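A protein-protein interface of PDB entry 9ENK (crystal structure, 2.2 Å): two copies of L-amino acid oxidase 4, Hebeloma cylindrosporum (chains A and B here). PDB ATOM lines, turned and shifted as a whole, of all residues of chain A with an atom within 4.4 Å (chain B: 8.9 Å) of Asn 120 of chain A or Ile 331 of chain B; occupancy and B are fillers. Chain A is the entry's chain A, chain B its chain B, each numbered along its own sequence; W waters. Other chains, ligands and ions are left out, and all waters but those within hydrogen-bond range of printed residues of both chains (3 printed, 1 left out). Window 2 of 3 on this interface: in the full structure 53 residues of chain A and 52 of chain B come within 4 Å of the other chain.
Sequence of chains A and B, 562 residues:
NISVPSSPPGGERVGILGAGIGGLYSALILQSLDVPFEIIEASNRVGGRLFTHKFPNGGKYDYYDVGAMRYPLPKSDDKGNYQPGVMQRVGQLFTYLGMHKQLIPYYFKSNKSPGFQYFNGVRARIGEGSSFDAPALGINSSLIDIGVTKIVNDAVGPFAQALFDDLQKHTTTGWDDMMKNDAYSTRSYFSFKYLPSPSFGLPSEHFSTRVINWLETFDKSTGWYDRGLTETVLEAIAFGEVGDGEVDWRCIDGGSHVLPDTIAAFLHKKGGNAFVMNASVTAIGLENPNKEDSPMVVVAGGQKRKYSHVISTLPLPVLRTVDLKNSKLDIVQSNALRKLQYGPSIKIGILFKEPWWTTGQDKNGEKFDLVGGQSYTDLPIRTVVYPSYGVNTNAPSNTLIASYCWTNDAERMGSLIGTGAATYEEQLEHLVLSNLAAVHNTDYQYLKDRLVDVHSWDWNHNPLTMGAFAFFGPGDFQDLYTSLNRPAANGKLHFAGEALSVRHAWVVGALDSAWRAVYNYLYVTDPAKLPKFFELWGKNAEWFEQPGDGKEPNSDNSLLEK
O of Asp 378 of chain A sits at hydrogen-bond distance from NH2 of Arg 320 of chain B, 2.7 Å away.
The side-chain amide oxygen (OD1) of Asn 120 of chain A is in hydrogen-bond range of the side-chain amide nitrogen (ND2) of Asn 335 of chain B, 3.1 Å away.
The backbone NH (N) of Asn 120 of chain A is in hydrogen-bond range of the side-chain carboxylate (OD2) of Asp 378 of chain A (2.9 Å).
ND2 of Asn 335 of chain B sits at hydrogen-bond distance from O of Ile 331 of chain B (2.8 Å).
The guanidinium group (NH2) of Arg 338 of chain B is in hydrogen-bond range of the side-chain amide oxygen (OD1) of Asn 335 of chain B (3.4 Å).
The side-chain amide nitrogen of Asn 120 of chain A sits at hydrogen-bond distance from the backbone carbonyl oxygen of Phe 132 of chain A, 2.9 Å away.
O of Ile 331 of chain B is in hydrogen-bond range of OG of Ser 334 of chain B, 3.1 Å away.
Asn 120 of chain A touches Ile 331 of chain B.
O of Asp 133 of chain A touches CD1 of Ile 331 of chain B (3.4 Å).
Ala 136 of chain A touches Ile 331 of chain B (O to CG2, 3.6 Å).
CG of Leu 137 of chain A touches CD1 of Ile 331 of chain B, 3.7 Å away.
Arg 338 of chain B touches Asp 378 of chain A (CD to O, 3.4 Å).
Of chain B, only Ile 331 and Asn 335 come within 4 Å of Asn 120 of chain A.
No residue of chain B comes within 4 Å of Gly 121 of chain A.
Printed residues of chain B within 4 Å of Asp 133 of chain A: Ile 331 (3.4 Å).
Of the printed residues of chain B, Asp 378 of chain A touches Arg 320 (2.7 Å) and Arg 338 (3.4 Å).
Printed residues of chain A within 4 Å of Ile 331 of chain B: Asn 120 (3.4 Å), Asp 133 (3.4 Å), Ala 136 (3.6 Å) and Leu 137 (3.7 Å).
Printed residues of chain A within 4 Å of Arg 338 of chain B: Asp 378.
Arg 486 of chain B touches none of the printed residues of chain A.
The nearest printed residue of chain B that does not touch Leu 137 of chain A is Asn 335 of chain B (4.01 Å).
Of the 16 printed residues of chain B, 4 touch a printed residue of chain A.
Hydrophobic or aromatic side chains of chain B within 4 Å of the printed part of chain A: Ile 331.
Of the 9 printed residues of chain A, 5 touch a printed residue of chain B.
Hydrophobic or aromatic side chains of chain A within 4 Å of the printed part of chain B: Ala 136 and Leu 137.
Among the printed residues, 7 pairs touch across the chains.
Among the printed residues, no Asp or Glu carboxylate lies within 4 Å of a Lys or Arg side-chain nitrogen of the other chain.
No position is printed for both chains.
Of the 7 pairs that touch across the chains among the printed residues, none has its exchanged pair printed and touching as well.
Water W2 lies within hydrogen-bond range of the side-chain amide oxygen (OD1) of Asn 120 of chain A (2.6 Å), the side-chain hydroxyl (OG) of Ser 334 of chain B (2.8 Å) and the side-chain amide nitrogen (ND2) of Asn 335 of chain B (3.5 Å).
Water W1 lies within hydrogen-bond range of NE of Arg 338 of chain B and OD2 of Asp 378 of chain A.
Water W3 lies within hydrogen-bond range of the side-chain carboxylate of Asp 378 of chain A and the guanidinium group of Arg 320 of chain B.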
ATOM      1  N   PHE A 119     -12.425   3.158   7.718  1.00  0.00           N
ATOM      2  CA  PHE A 119     -11.147   2.459   7.718  1.00  0.00           C
ATOM      3  C   PHE A 119     -11.354   1.005   8.130  1.00  0.00           C
ATOM      4  O   PHE A 119     -12.075   0.720   9.090  1.00  0.00           O
ATOM      5  CB  PHE A 119     -10.141   3.119   8.679  1.00  0.00           C
ATOM      6  CG  PHE A 119      -9.700   4.482   8.254  1.00  0.00           C
ATOM      7  CD1 PHE A 119     -10.493   5.593   8.506  1.00  0.00           C
ATOM      8  CD2 PHE A 119      -8.492   4.660   7.598  1.00  0.00           C
ATOM      9  CE1 PHE A 119     -10.089   6.856   8.109  1.00  0.00           C
ATOM     10  CE2 PHE A 119      -8.088   5.921   7.193  1.00  0.00           C
ATOM     11  CZ  PHE A 119      -8.883   7.016   7.448  1.00  0.00           C
ATOM     12  N   ASN A 120     -10.705   0.097   7.408  1.00  0.00           N
ATOM     13  CA  ASN A 120     -10.768  -1.336   7.699  1.00  0.00           C
ATOM     14  C   ASN A 120     -12.203  -1.847   7.724  1.00  0.00           C
ATOM     15  O   ASN A 120     -12.555  -2.720   8.517  1.00  0.00           O
ATOM     16  CB  ASN A 120     -10.065  -1.642   9.022  1.00  0.00           C
ATOM     17  CG  ASN A 120      -8.626  -1.201   9.023  1.00  0.00           C
ATOM     18  OD1 ASN A 120      -7.882  -1.489   8.090  1.00  0.00           O
ATOM     19  ND2 ASN A 120      -8.227  -0.483  10.058  1.00  0.00           N
ATOM     20  N   GLY A 121     -13.039  -1.304   6.843  1.00  0.00           N
ATOM     21  CA  GLY A 121     -14.425  -1.708   6.754  1.00  0.00           C
ATOM     22  C   GLY A 121     -15.317  -1.180   7.852  1.00  0.00           C
ATOM     23  O   GLY A 121     -16.501  -1.546   7.901  1.00  0.00           O
ATOM     24  N   VAL A 122     -14.798  -0.333   8.732  1.00  0.00           N
ATOM     25  CA  VAL A 122     -15.553   0.224   9.848  1.00  0.00           C
ATOM     26  C   VAL A 122     -15.856   1.684   9.550  1.00  0.00           C
ATOM     27  O   VAL A 122     -14.952   2.456   9.199  1.00  0.00           O
ATOM     28  CB  VAL A 122     -14.785   0.080  11.171  1.00  0.00           C
ATOM     29  CG1 VAL A 122     -15.556   0.727  12.310  1.00  0.00           C
ATOM     30  CG2 VAL A 122     -14.533  -1.395  11.466  1.00  0.00           C
ATOM     31  N   PHE A 132     -11.552   1.378  14.640  1.00  0.00           N
ATOM     32  CA  PHE A 132     -11.491   0.888  13.263  1.00  0.00           C
ATOM     33  C   PHE A 132     -10.787  -0.462  13.190  1.00  0.00           C
ATOM     34  O   PHE A 132      -9.922  -0.700  12.346  1.00  0.00           O
ATOM     35  CB  PHE A 132     -10.812   1.918  12.361  1.00  0.00           C
ATOM     36  CG  PHE A 132     -11.450   3.274  12.422  1.00  0.00           C
ATOM     37  CD1 PHE A 132     -12.583   3.556  11.678  1.00  0.00           C
ATOM     38  CD2 PHE A 132     -10.925   4.269  13.232  1.00  0.00           C
ATOM     39  CE1 PHE A 132     -13.183   4.802  11.743  1.00  0.00           C
ATOM     40  CE2 PHE A 132     -11.516   5.513  13.288  1.00  0.00           C
ATOM     41  CZ  PHE A 132     -12.651   5.775  12.551  1.00  0.00           C
ATOM     42  N   ASP A 133     -11.181  -1.356  14.094  1.00  0.00           N
ATOM     43  CA  ASP A 133     -10.706  -2.739  14.134  1.00  0.00           C
ATOM     44  C   ASP A 133      -9.200  -2.827  14.386  1.00  0.00           C
ATOM     45  O   ASP A 133      -8.588  -3.869  14.129  1.00  0.00           O
ATOM     46  CB  ASP A 133     -11.077  -3.468  12.833  1.00  0.00           C
ATOM     47  CG  ASP A 133     -11.519  -4.911  13.058  1.00  0.00           C
ATOM     48  OD1 ASP A 133     -11.851  -5.285  14.202  1.00  0.00           O
ATOM     49  OD2 ASP A 133     -11.517  -5.687  12.073  1.00  0.00           O
ATOM     50  N   ALA A 136      -7.543  -5.966  15.786  1.00  0.00           N
ATOM     51  CA  ALA A 136      -7.268  -7.039  14.841  1.00  0.00           C
ATOM     52  C   ALA A 136      -5.957  -6.821  14.099  1.00  0.00           C
ATOM     53  O   ALA A 136      -5.372  -7.791  13.607  1.00  0.00           O
ATOM     54  CB  ALA A 136      -8.429  -7.176  13.851  1.00  0.00           C
ATOM     55  N   LEU A 137      -5.493  -5.570  13.992  1.00  0.00           N
ATOM     56  CA  LEU A 137      -4.203  -5.286  13.381  1.00  0.00           C
ATOM     57  C   LEU A 137      -3.037  -5.564  14.316  1.00  0.00           C
ATOM     58  O   LEU A 137      -1.887  -5.525  13.874  1.00  0.00           O
ATOM     59  CB  LEU A 137      -4.115  -3.826  12.929  1.00  0.00           C
ATOM     60  CG  LEU A 137      -4.358  -3.487  11.465  1.00  0.00           C
ATOM     61  CD1 LEU A 137      -4.348  -1.967  11.291  1.00  0.00           C
ATOM     62  CD2 LEU A 137      -3.330  -4.127  10.541  1.00  0.00           C
ATOM     63  N   ASP A 378      -9.488   4.834   4.082  1.00  0.00           N
ATOM     64  CA  ASP A 378      -8.343   4.149   3.498  1.00  0.00           C
ATOM     65  C   ASP A 378      -8.641   3.633   2.090  1.00  0.00           C
ATOM     66  O   ASP A 378      -7.756   3.036   1.464  1.00  0.00           O
ATOM     67  CB  ASP A 378      -7.873   3.006   4.409  1.00  0.00           C
ATOM     68  CG  ASP A 378      -8.981   2.032   4.773  1.00  0.00           C
ATOM     69  OD1 ASP A 378     -10.090   2.119   4.204  1.00  0.00           O
ATOM     70  OD2 ASP A 378      -8.731   1.161   5.647  1.00  0.00           O
ATOM     71  N   ARG B 320      -6.860  -2.861  -5.851  1.00  0.00           N
ATOM     72  CA  ARG B 320      -7.526  -1.815  -5.085  1.00  0.00           C
ATOM     73  C   ARG B 320      -8.659  -1.158  -5.861  1.00  0.00           C
ATOM     74  O   ARG B 320      -9.502  -0.502  -5.245  1.00  0.00           O
ATOM     75  CB  ARG B 320      -6.503  -0.767  -4.637  1.00  0.00           C
ATOM     76  CG  ARG B 320      -5.557  -1.261  -3.539  1.00  0.00           C
ATOM     77  CD  ARG B 320      -6.071  -0.879  -2.152  1.00  0.00           C
ATOM     78  NE  ARG B 320      -6.033   0.571  -1.968  1.00  0.00           N
ATOM     79  CZ  ARG B 320      -6.684   1.232  -1.019  1.00  0.00           C
ATOM     80  NH1 ARG B 320      -7.445   0.603  -0.140  1.00  0.00           N
ATOM     81  NH2 ARG B 320      -6.551   2.560  -0.944  1.00  0.00           N
ATOM     82  N   LYS B 328     -13.308 -11.645   1.591  1.00  0.00           N
ATOM     83  CA  LYS B 328     -12.969 -11.858   2.999  1.00  0.00           C
ATOM     84  C   LYS B 328     -11.468 -11.742   3.252  1.00  0.00           C
ATOM     85  O   LYS B 328     -10.853 -12.581   3.909  1.00  0.00           O
ATOM     86  CB  LYS B 328     -13.493 -13.224   3.465  1.00  0.00           C
ATOM     87  CG  LYS B 328     -15.005 -13.363   3.367  1.00  0.00           C
ATOM     88  CD  LYS B 328     -15.492 -14.755   3.782  1.00  0.00           C
ATOM     89  CE  LYS B 328     -15.237 -15.038   5.263  1.00  0.00           C
ATOM     90  NZ  LYS B 328     -15.865 -16.321   5.708  1.00  0.00           N
ATOM     91  N   LEU B 329     -10.869 -10.676   2.728  1.00  0.00           N
ATOM     92  CA  LEU B 329      -9.492 -10.369   3.094  1.00  0.00           C
ATOM     93  C   LEU B 329      -9.426 -10.019   4.577  1.00  0.00           C
ATOM     94  O   LEU B 329     -10.299  -9.329   5.104  1.00  0.00           O
ATOM     95  CB  LEU B 329      -8.946  -9.215   2.257  1.00  0.00           C
ATOM     96  CG  LEU B 329      -8.440  -9.559   0.858  1.00  0.00           C
ATOM     97  CD1 LEU B 329      -9.572 -10.068  -0.041  1.00  0.00           C
ATOM     98  CD2 LEU B 329      -7.745  -8.343   0.254  1.00  0.00           C
ATOM     99  N   ASP B 330      -8.399 -10.510   5.263  1.00  0.00           N
ATOM    100  CA  ASP B 330      -8.231 -10.083   6.642  1.00  0.00           C
ATOM    101  C   ASP B 330      -7.622  -8.682   6.659  1.00  0.00           C
ATOM    102  O   ASP B 330      -7.148  -8.160   5.640  1.00  0.00           O
ATOM    103  CB  ASP B 330      -7.392 -11.082   7.445  1.00  0.00           C
ATOM    104  CG  ASP B 330      -5.934 -11.148   6.994  1.00  0.00           C
ATOM    105  OD1 ASP B 330      -5.277 -10.094   6.903  1.00  0.00           O
ATOM    106  OD2 ASP B 330      -5.431 -12.269   6.779  1.00  0.00           O
ATOM    107  N   ILE B 331      -7.638  -8.066   7.839  1.00  0.00           N
ATOM    108  CA  ILE B 331      -7.287  -6.654   7.947  1.00  0.00           C
ATOM    109  C   ILE B 331      -5.859  -6.405   7.494  1.00  0.00           C
ATOM    110  O   ILE B 331      -5.550  -5.331   6.970  1.00  0.00           O
ATOM    111  CB  ILE B 331      -7.520  -6.172   9.392  1.00  0.00           C
ATOM    112  CG1 ILE B 331      -7.339  -4.660   9.489  1.00  0.00           C
ATOM    113  CG2 ILE B 331      -6.585  -6.900  10.363  1.00  0.00           C
ATOM    114  CD1 ILE B 331      -7.931  -4.084  10.781  1.00  0.00           C
ATOM    115  N   VAL B 332      -4.964  -7.380   7.675  1.00  0.00           N
ATOM    116  CA  VAL B 332      -3.588  -7.188   7.220  1.00  0.00           C
ATOM    117  C   VAL B 332      -3.519  -7.264   5.697  1.00  0.00           C
ATOM    118  O   VAL B 332      -2.865  -6.442   5.053  1.00  0.00           O
ATOM    119  CB  VAL B 332      -2.651  -8.215   7.884  1.00  0.00           C
ATOM    120  CG1 VAL B 332      -1.201  -7.921   7.532  1.00  0.00           C
ATOM    121  CG2 VAL B 332      -2.840  -8.210   9.383  1.00  0.00           C
ATOM    122  N   GLN B 333      -4.216  -8.231   5.097  1.00  0.00           N
ATOM    123  CA  GLN B 333      -4.217  -8.344   3.643  1.00  0.00           C
ATOM    124  C   GLN B 333      -4.758  -7.078   2.987  1.00  0.00           C
ATOM    125  O   GLN B 333      -4.180  -6.575   2.011  1.00  0.00           O
ATOM    126  CB  GLN B 333      -5.034  -9.555   3.212  1.00  0.00           C
ATOM    127  CG  GLN B 333      -4.436 -10.898   3.630  1.00  0.00           C
ATOM    128  CD  GLN B 333      -5.366 -12.058   3.312  1.00  0.00           C
ATOM    129  OE1 GLN B 333      -6.571 -11.979   3.549  1.00  0.00           O
ATOM    130  NE2 GLN B 333      -4.809 -13.133   2.754  1.00  0.00           N
ATOM    131  N   SER B 334      -5.863  -6.541   3.508  1.00  0.00           N
ATOM    132  CA  SER B 334      -6.421  -5.332   2.912  1.00  0.00           C
ATOM    133  C   SER B 334      -5.495  -4.128   3.113  1.00  0.00           C
ATOM    134  O   SER B 334      -5.381  -3.276   2.229  1.00  0.00           O
ATOM    135  CB  SER B 334      -7.825  -5.062   3.468  1.00  0.00           C
ATOM    136  OG  SER B 334      -7.828  -4.925   4.879  1.00  0.00           O
ATOM    137  N   ASN B 335      -4.814  -4.046   4.258  1.00  0.00           N
ATOM    138  CA  ASN B 335      -3.786  -3.020   4.424  1.00  0.00           C
ATOM    139  C   ASN B 335      -2.647  -3.214   3.425  1.00  0.00           C
ATOM    140  O   ASN B 335      -2.125  -2.244   2.858  1.00  0.00           O
ATOM    141  CB  ASN B 335      -3.230  -3.048   5.852  1.00  0.00           C
ATOM    142  CG  ASN B 335      -3.986  -2.144   6.798  1.00  0.00           C
ATOM    143  OD1 ASN B 335      -3.556  -1.032   7.079  1.00  0.00           O
ATOM    144  ND2 ASN B 335      -5.129  -2.616   7.288  1.00  0.00           N
ATOM    145  N   ALA B 336      -2.248  -4.465   3.197  1.00  0.00           N
ATOM    146  CA  ALA B 336      -1.115  -4.727   2.316  1.00  0.00           C
ATOM    147  C   ALA B 336      -1.395  -4.259   0.892  1.00  0.00           C
ATOM    148  O   ALA B 336      -0.496  -3.743   0.221  1.00  0.00           O
ATOM    149  CB  ALA B 336      -0.769  -6.214   2.339  1.00  0.00           C
ATOM    150  N   LEU B 337      -2.626  -4.458   0.400  1.00  0.00           N
ATOM    151  CA  LEU B 337      -2.943  -4.035  -0.961  1.00  0.00           C
ATOM    152  C   LEU B 337      -2.681  -2.542  -1.148  1.00  0.00           C
ATOM    153  O   LEU B 337      -2.256  -2.111  -2.221  1.00  0.00           O
ATOM    154  CB  LEU B 337      -4.395  -4.356  -1.297  1.00  0.00           C
ATOM    155  CG  LEU B 337      -4.809  -5.826  -1.378  1.00  0.00           C
ATOM    156  CD1 LEU B 337      -6.262  -5.908  -1.841  1.00  0.00           C
ATOM    157  CD2 LEU B 337      -3.900  -6.609  -2.301  1.00  0.00           C
ATOM    158  N   ARG B 338      -2.923  -1.743  -0.110  1.00  0.00           N
ATOM    159  CA  ARG B 338      -2.752  -0.301  -0.217  1.00  0.00           C
ATOM    160  C   ARG B 338      -1.307   0.133   0.006  1.00  0.00           C
ATOM    161  O   ARG B 338      -0.787   0.979  -0.736  1.00  0.00           O
ATOM    162  CB  ARG B 338      -3.667   0.403   0.792  1.00  0.00           C
ATOM    163  CG  ARG B 338      -3.479   1.911   0.880  1.00  0.00           C
ATOM    164  CD  ARG B 338      -4.416   2.531   1.892  1.00  0.00           C
ATOM    165  NE  ARG B 338      -4.195   1.984   3.223  1.00  0.00           N
ATOM    166  CZ  ARG B 338      -3.264   2.401   4.066  1.00  0.00           C
ATOM    167  NH1 ARG B 338      -2.432   3.385   3.749  1.00  0.00           N
ATOM    168  NH2 ARG B 338      -3.167   1.823   5.260  1.00  0.00           N
ATOM    169  N   LEU B 480       4.003  -6.448   6.078  1.00  0.00           N
ATOM    170  CA  LEU B 480       2.813  -6.721   5.290  1.00  0.00           C
ATOM    171  C   LEU B 480       2.982  -7.769   4.205  1.00  0.00           C
ATOM    172  O   LEU B 480       1.977  -8.302   3.739  1.00  0.00           O
ATOM    173  CB  LEU B 480       2.321  -5.423   4.629  1.00  0.00           C
ATOM    174  CG  LEU B 480       1.946  -4.308   5.599  1.00  0.00           C
ATOM    175  CD1 LEU B 480       1.880  -2.964   4.892  1.00  0.00           C
ATOM    176  CD2 LEU B 480       0.630  -4.629   6.274  1.00  0.00           C
ATOM    177  N   SER B 483       1.326 -11.427   4.519  1.00  0.00           N
ATOM    178  CA  SER B 483      -0.127 -11.566   4.575  1.00  0.00           C
ATOM    179  C   SER B 483      -0.710 -11.959   3.224  1.00  0.00           C
ATOM    180  O   SER B 483      -1.716 -12.676   3.162  1.00  0.00           O
ATOM    181  CB  SER B 483      -0.773 -10.268   5.059  1.00  0.00           C
ATOM    182  OG  SER B 483      -0.728  -9.261   4.066  1.00  0.00           O
ATOM    183  N   LEU B 484      -0.106 -11.508   2.129  1.00  0.00           N
ATOM    184  CA  LEU B 484      -0.658 -11.805   0.815  1.00  0.00           C
ATOM    185  C   LEU B 484      -0.199 -13.150   0.278  1.00  0.00           C
ATOM    186  O   LEU B 484      -0.741 -13.610  -0.734  1.00  0.00           O
ATOM    187  CB  LEU B 484      -0.312 -10.694  -0.177  1.00  0.00           C
ATOM    188  CG  LEU B 484      -0.979  -9.346   0.101  1.00  0.00           C
ATOM    189  CD1 LEU B 484      -0.549  -8.302  -0.926  1.00  0.00           C
ATOM    190  CD2 LEU B 484      -2.497  -9.483   0.108  1.00  0.00           C
ATOM    191  N   ARG B 486      -0.730 -15.695   2.192  1.00  0.00           N
ATOM    192  CA  ARG B 486      -1.872 -16.478   2.633  1.00  0.00           C
ATOM    193  C   ARG B 486      -3.050 -16.207   1.700  1.00  0.00           C
ATOM    194  O   ARG B 486      -3.205 -15.092   1.195  1.00  0.00           O
ATOM    195  CB  ARG B 486      -2.260 -16.118   4.062  1.00  0.00           C
ATOM    196  CG  ARG B 486      -1.127 -16.225   5.073  1.00  0.00           C
ATOM    197  CD  ARG B 486      -1.662 -16.085   6.511  1.00  0.00           C
ATOM    198  NE  ARG B 486      -2.396 -14.840   6.705  1.00  0.00           N
ATOM    199  CZ  ARG B 486      -1.850 -13.708   7.134  1.00  0.00           C
ATOM    200  NH1 ARG B 486      -0.558 -13.633   7.439  1.00  0.00           N
ATOM    201  NH2 ARG B 486      -2.613 -12.620   7.250  1.00  0.00           N
HETATM  202  O   HOH W   1      -5.891  -0.066   4.219  1.00  0.00           O
HETATM  203  O   HOH W   2      -8.182  -2.314   5.668  1.00  0.00           O
HETATM  204  O   HOH W   3      -9.473   0.319   2.001  1.00  0.00           O
